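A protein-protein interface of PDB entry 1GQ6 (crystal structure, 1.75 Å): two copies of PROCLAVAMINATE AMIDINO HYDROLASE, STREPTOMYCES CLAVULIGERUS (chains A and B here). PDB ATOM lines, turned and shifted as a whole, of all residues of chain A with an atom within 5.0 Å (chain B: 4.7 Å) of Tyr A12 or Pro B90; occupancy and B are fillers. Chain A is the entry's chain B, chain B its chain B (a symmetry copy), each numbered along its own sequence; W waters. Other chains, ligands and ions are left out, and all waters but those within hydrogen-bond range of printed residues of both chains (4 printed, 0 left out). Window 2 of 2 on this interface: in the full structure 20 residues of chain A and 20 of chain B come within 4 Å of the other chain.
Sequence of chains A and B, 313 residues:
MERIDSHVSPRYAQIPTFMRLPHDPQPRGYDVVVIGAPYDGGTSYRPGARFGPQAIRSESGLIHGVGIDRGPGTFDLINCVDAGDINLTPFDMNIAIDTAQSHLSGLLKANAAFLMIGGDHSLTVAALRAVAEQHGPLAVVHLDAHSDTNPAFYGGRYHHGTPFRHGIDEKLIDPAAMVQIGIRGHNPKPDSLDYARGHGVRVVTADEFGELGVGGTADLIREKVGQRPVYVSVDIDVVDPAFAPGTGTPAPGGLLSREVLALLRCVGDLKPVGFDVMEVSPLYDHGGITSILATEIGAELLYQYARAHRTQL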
ATOM      1  N   PRO A  10       7.701  26.019  -9.595  1.00  0.00           N
ATOM      2  CA  PRO A  10       7.510  27.448  -9.388  1.00  0.00           C
ATOM      3  C   PRO A  10       6.019  27.775  -9.330  1.00  0.00           C
ATOM      4  O   PRO A  10       5.184  27.050  -9.881  1.00  0.00           O
ATOM      5  CB  PRO A  10       8.222  28.078 -10.576  1.00  0.00           C
ATOM      6  CG  PRO A  10       8.578  26.980 -11.493  1.00  0.00           C
ATOM      7  CD  PRO A  10       8.510  25.712 -10.788  1.00  0.00           C
ATOM      8  N   ARG A  11       5.686  28.875  -8.672  1.00  0.00           N
ATOM      9  CA  ARG A  11       4.315  29.203  -8.362  1.00  0.00           C
ATOM     10  C   ARG A  11       3.474  29.580  -9.583  1.00  0.00           C
ATOM     11  O   ARG A  11       2.271  29.494  -9.533  1.00  0.00           O
ATOM     12  CB  ARG A  11       4.266  30.327  -7.325  1.00  0.00           C
ATOM     13  CG  ARG A  11       4.799  29.900  -5.964  1.00  0.00           C
ATOM     14  CD  ARG A  11       4.943  31.058  -5.011  1.00  0.00           C
ATOM     15  NE  ARG A  11       6.194  31.770  -5.250  1.00  0.00           N
ATOM     16  CZ  ARG A  11       6.567  32.861  -4.592  1.00  0.00           C
ATOM     17  NH1 ARG A  11       5.786  33.386  -3.638  1.00  0.00           N
ATOM     18  NH2 ARG A  11       7.737  33.402  -4.850  1.00  0.00           N
ATOM     19  N   TYR A  12       4.120  29.943 -10.684  1.00  0.00           N
ATOM     20  CA  TYR A  12       3.404  30.282 -11.937  1.00  0.00           C
ATOM     21  C   TYR A  12       3.218  29.058 -12.822  1.00  0.00           C
ATOM     22  O   TYR A  12       2.568  29.155 -13.854  1.00  0.00           O
ATOM     23  CB  TYR A  12       4.189  31.364 -12.724  1.00  0.00           C
ATOM     24  CG  TYR A  12       5.634  31.038 -12.835  1.00  0.00           C
ATOM     25  CD1 TYR A  12       6.094  30.131 -13.781  1.00  0.00           C
ATOM     26  CD2 TYR A  12       6.579  31.613 -11.988  1.00  0.00           C
ATOM     27  CE1 TYR A  12       7.438  29.790 -13.861  1.00  0.00           C
ATOM     28  CE2 TYR A  12       7.904  31.274 -12.059  1.00  0.00           C
ATOM     29  CZ  TYR A  12       8.356  30.361 -12.977  1.00  0.00           C
ATOM     30  OH  TYR A  12       9.686  30.027 -13.036  1.00  0.00           O
ATOM     31  N   ALA A  13       3.787  27.914 -12.445  1.00  0.00           N
ATOM     32  CA  ALA A  13       3.691  26.700 -13.260  1.00  0.00           C
ATOM     33  C   ALA A  13       2.366  25.986 -12.957  1.00  0.00           C
ATOM     34  O   ALA A  13       1.815  26.157 -11.879  1.00  0.00           O
ATOM     35  CB  ALA A  13       4.875  25.777 -12.968  1.00  0.00           C
ATOM     36  N   GLN A  14       1.870  25.245 -13.944  1.00  0.00           N
ATOM     37  CA  GLN A  14       0.615  24.498 -13.914  1.00  0.00           C
ATOM     38  C   GLN A  14      -0.618  25.341 -14.189  1.00  0.00           C
ATOM     39  O   GLN A  14      -0.585  26.560 -14.132  1.00  0.00           O
ATOM     40  CB  GLN A  14       0.469  23.632 -12.639  1.00  0.00           C
ATOM     41  CG  GLN A  14       1.701  22.807 -12.372  1.00  0.00           C
ATOM     42  CD  GLN A  14       2.104  21.905 -13.533  1.00  0.00           C
ATOM     43  OE1 GLN A  14       1.266  21.539 -14.369  1.00  0.00           O
ATOM     44  NE2 GLN A  14       3.372  21.517 -13.569  1.00  0.00           N
ATOM     45  N   PRO B  38       6.923  26.590 -18.954  1.00  0.00           N
ATOM     46  CA  PRO B  38       6.963  27.948 -18.380  1.00  0.00           C
ATOM     47  C   PRO B  38       8.347  28.316 -17.883  1.00  0.00           C
ATOM     48  O   PRO B  38       8.634  28.215 -16.695  1.00  0.00           O
ATOM     49  CB  PRO B  38       5.938  27.887 -17.268  1.00  0.00           C
ATOM     50  CG  PRO B  38       5.993  26.455 -16.764  1.00  0.00           C
ATOM     51  CD  PRO B  38       6.257  25.625 -18.051  1.00  0.00           C
ATOM     52  N   ARG B  50       8.250  32.972 -19.253  1.00  0.00           N
ATOM     53  CA  ARG B  50       7.837  31.963 -18.299  1.00  0.00           C
ATOM     54  C   ARG B  50       6.312  31.993 -18.094  1.00  0.00           C
ATOM     55  O   ARG B  50       5.727  30.998 -17.633  1.00  0.00           O
ATOM     56  CB  ARG B  50       8.536  32.114 -16.943  1.00  0.00           C
ATOM     57  CG  ARG B  50       8.090  33.312 -16.099  1.00  0.00           C
ATOM     58  CD  ARG B  50       8.861  33.534 -14.805  1.00  0.00           C
ATOM     59  NE  ARG B  50      10.274  33.781 -15.077  1.00  0.00           N
ATOM     60  CZ  ARG B  50      11.240  33.813 -14.174  1.00  0.00           C
ATOM     61  NH1 ARG B  50      10.990  33.714 -12.873  1.00  0.00           N
ATOM     62  NH2 ARG B  50      12.486  34.011 -14.578  1.00  0.00           N
ATOM     63  N   PHE B  51       5.695  33.143 -18.394  1.00  0.00           N
ATOM     64  CA  PHE B  51       4.248  33.313 -18.286  1.00  0.00           C
ATOM     65  C   PHE B  51       3.539  33.026 -19.600  1.00  0.00           C
ATOM     66  O   PHE B  51       2.327  33.129 -19.684  1.00  0.00           O
ATOM     67  CB  PHE B  51       3.912  34.726 -17.802  1.00  0.00           C
ATOM     68  CG  PHE B  51       4.258  34.958 -16.371  1.00  0.00           C
ATOM     69  CD1 PHE B  51       3.506  34.379 -15.373  1.00  0.00           C
ATOM     70  CD2 PHE B  51       5.346  35.745 -16.021  1.00  0.00           C
ATOM     71  CE1 PHE B  51       3.825  34.564 -14.047  1.00  0.00           C
ATOM     72  CE2 PHE B  51       5.680  35.887 -14.686  1.00  0.00           C
ATOM     73  CZ  PHE B  51       4.907  35.312 -13.708  1.00  0.00           C
ATOM     74  N   GLN B  54       0.715  30.315 -19.348  1.00  0.00           N
ATOM     75  CA  GLN B  54      -0.451  30.785 -18.596  1.00  0.00           C
ATOM     76  C   GLN B  54      -1.272  31.756 -19.455  1.00  0.00           C
ATOM     77  O   GLN B  54      -2.503  31.670 -19.548  1.00  0.00           O
ATOM     78  CB  GLN B  54       0.009  31.457 -17.287  1.00  0.00           C
ATOM     79  CG  GLN B  54      -1.097  31.776 -16.318  1.00  0.00           C
ATOM     80  CD  GLN B  54      -0.583  32.566 -15.105  1.00  0.00           C
ATOM     81  OE1 GLN B  54      -0.326  33.771 -15.206  1.00  0.00           O
ATOM     82  NE2 GLN B  54      -0.368  31.872 -13.988  1.00  0.00           N
ATOM     83  N   ASP B  85       1.890  21.687 -17.237  1.00  0.00           N
ATOM     84  CA  ASP B  85       3.235  22.183 -17.513  1.00  0.00           C
ATOM     85  C   ASP B  85       4.356  21.256 -17.037  1.00  0.00           C
ATOM     86  O   ASP B  85       4.152  20.403 -16.169  1.00  0.00           O
ATOM     87  CB  ASP B  85       3.478  23.488 -16.759  1.00  0.00           C
ATOM     88  CG  ASP B  85       2.684  24.640 -17.289  1.00  0.00           C
ATOM     89  OD1 ASP B  85       2.154  24.560 -18.443  1.00  0.00           O
ATOM     90  OD2 ASP B  85       2.539  25.662 -16.593  1.00  0.00           O
ATOM     91  N   LEU B  88       9.700  23.455 -14.562  1.00  0.00           N
ATOM     92  CA  LEU B  88      11.005  23.987 -14.959  1.00  0.00           C
ATOM     93  C   LEU B  88      11.504  25.040 -13.985  1.00  0.00           C
ATOM     94  O   LEU B  88      10.899  26.087 -13.761  1.00  0.00           O
ATOM     95  CB  LEU B  88      10.916  24.565 -16.359  1.00  0.00           C
ATOM     96  CG  LEU B  88      10.504  23.568 -17.416  1.00  0.00           C
ATOM     97  CD1 LEU B  88      10.200  24.279 -18.730  1.00  0.00           C
ATOM     98  CD2 LEU B  88      11.579  22.531 -17.594  1.00  0.00           C
ATOM     99  N   THR B  89      12.638  24.736 -13.382  1.00  0.00           N
ATOM    100  CA  THR B  89      13.198  25.695 -12.442  1.00  0.00           C
ATOM    101  C   THR B  89      13.625  26.961 -13.169  1.00  0.00           C
ATOM    102  O   THR B  89      14.166  26.897 -14.266  1.00  0.00           O
ATOM    103  CB  THR B  89      14.380  25.084 -11.751  1.00  0.00           C
ATOM    104  OG1 THR B  89      15.020  26.093 -10.986  1.00  0.00           O
ATOM    105  CG2 THR B  89      15.463  24.622 -12.758  1.00  0.00           C
ATOM    106  N   PRO B  90      13.382  28.119 -12.572  1.00  0.00           N
ATOM    107  CA  PRO B  90      13.889  29.371 -13.128  1.00  0.00           C
ATOM    108  C   PRO B  90      15.320  29.684 -12.693  1.00  0.00           C
ATOM    109  O   PRO B  90      15.825  30.725 -13.060  1.00  0.00           O
ATOM    110  CB  PRO B  90      12.978  30.409 -12.499  1.00  0.00           C
ATOM    111  CG  PRO B  90      12.606  29.838 -11.192  1.00  0.00           C
ATOM    112  CD  PRO B  90      12.566  28.356 -11.379  1.00  0.00           C
ATOM    113  N   PHE B  91      15.945  28.830 -11.904  1.00  0.00           N
ATOM    114  CA  PHE B  91      17.257  29.148 -11.309  1.00  0.00           C
ATOM    115  C   PHE B  91      18.465  28.466 -11.957  1.00  0.00           C
ATOM    116  O   PHE B  91      19.620  28.761 -11.586  1.00  0.00           O
ATOM    117  CB  PHE B  91      17.222  28.723  -9.870  1.00  0.00           C
ATOM    118  CG  PHE B  91      16.087  29.322  -9.087  1.00  0.00           C
ATOM    119  CD1 PHE B  91      15.884  30.677  -9.077  1.00  0.00           C
ATOM    120  CD2 PHE B  91      15.267  28.519  -8.334  1.00  0.00           C
ATOM    121  CE1 PHE B  91      14.833  31.229  -8.335  1.00  0.00           C
ATOM    122  CE2 PHE B  91      14.232  29.063  -7.588  1.00  0.00           C
ATOM    123  CZ  PHE B  91      14.015  30.413  -7.612  1.00  0.00           C
ATOM    124  N   ASP B  92      18.219  27.534 -12.883  1.00  0.00           N
ATOM    125  CA  ASP B  92      19.331  26.726 -13.441  1.00  0.00           C
ATOM    126  C   ASP B  92      19.011  26.258 -14.832  1.00  0.00           C
ATOM    127  O   ASP B  92      18.121  25.455 -15.033  1.00  0.00           O
ATOM    128  CB  ASP B  92      19.668  25.516 -12.579  1.00  0.00           C
ATOM    129  CG  ASP B  92      21.014  24.947 -12.900  1.00  0.00           C
ATOM    130  OD1 ASP B  92      21.151  24.225 -13.926  1.00  0.00           O
ATOM    131  OD2 ASP B  92      22.003  25.106 -12.130  1.00  0.00           O
HETATM  132  O   HOH W   1      10.681  28.515 -14.998  1.00  0.00           O
HETATM  133  O   HOH W   2       1.921  28.241 -16.527  1.00  0.00           O
HETATM  134  O   HOH W   3       2.229  18.518 -15.768  1.00  0.00           O
HETATM  135  O   HOH W   4      -0.271  29.048 -13.359  1.00  0.00           O
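N of Gln A14 lies within hydrogen-bond range of OD2 of Asp B85, 2.8 Å away.
Among the printed residues, merely in contact across the chains: Tyr A12 with Pro B90, Pro A10 with Leu B88, Tyr A12 with Pro B38, Tyr A12 with Phe B51, Ala A13 with Asp B85 and Tyr A12 with Arg B50.
Printed residues of chain B within 4 Å of Pro A10: Leu B88 (3.4 Å).
Of the printed residues of chain B, Tyr A12 touches Pro B38 (3.5 Å), Arg B50 (3.7 Å), Phe B51 (3.5 Å) and Pro B90 (3.4 Å).
Printed residues of chain B within 4 Å of Gln A14: Asp B85.
Of the printed residues of chain A, Arg B50 touches Tyr A12 (3.7 Å).
Printed residues of chain A within 4 Å of Leu B88: Pro A10.
Thr B89 touches none of the printed residues of chain A.
Of chain A, only Tyr A12 (3.4 Å) comes within 4 Å of Pro B90.
Phe B91 touches none of the printed residues of chain A.
The nearest printed residue of chain B that does not touch Pro A10 is Pro B90 (4.2 Å).
Of the 5 printed residues of chain A, 4 touch a printed residue of chain B.
Printed residues of chain A that touch a printed residue of chain B: Pro A10, Tyr A12, Ala A13 and Gln A14.
Hydrophobic or aromatic side chains of chain A within 4 Å of the printed part of chain B: Pro A10 and Tyr A12.
Printed residues of chain B that touch a printed residue of chain A: Pro B38, Arg B50, Phe B51, Asp B85, Leu B88 and Pro B90.
Among the printed residues, 7 pairs touch across the chains.
Among the printed residues, no Asp or Glu carboxylate lies within 4 Å of a Lys or Arg side-chain nitrogen of the other chain.
No position is printed for both chains.
Of the 7 pairs that touch across the chains among the printed residues, none has its exchanged pair printed and touching as well.
Water W4 lies within hydrogen-bond range of O of Gln A14 (2.6 Å), O of Tyr A12 (2.9 Å) and NE2 of Gln B54 (2.9 Å).
Water W2 lies within hydrogen-bond range of OD2 of Asp B85 and O of Tyr A12.
Water W1 lies within hydrogen-bond range of OH of Tyr A12 (2.7 Å), O of Pro B38 (2.7 Å) and O of Leu B88 (2.7 Å).
Water W3 lies within hydrogen-bond range of O of Asp B85 (2.7 Å) and OE1 of Gln A14 (3.5 Å).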
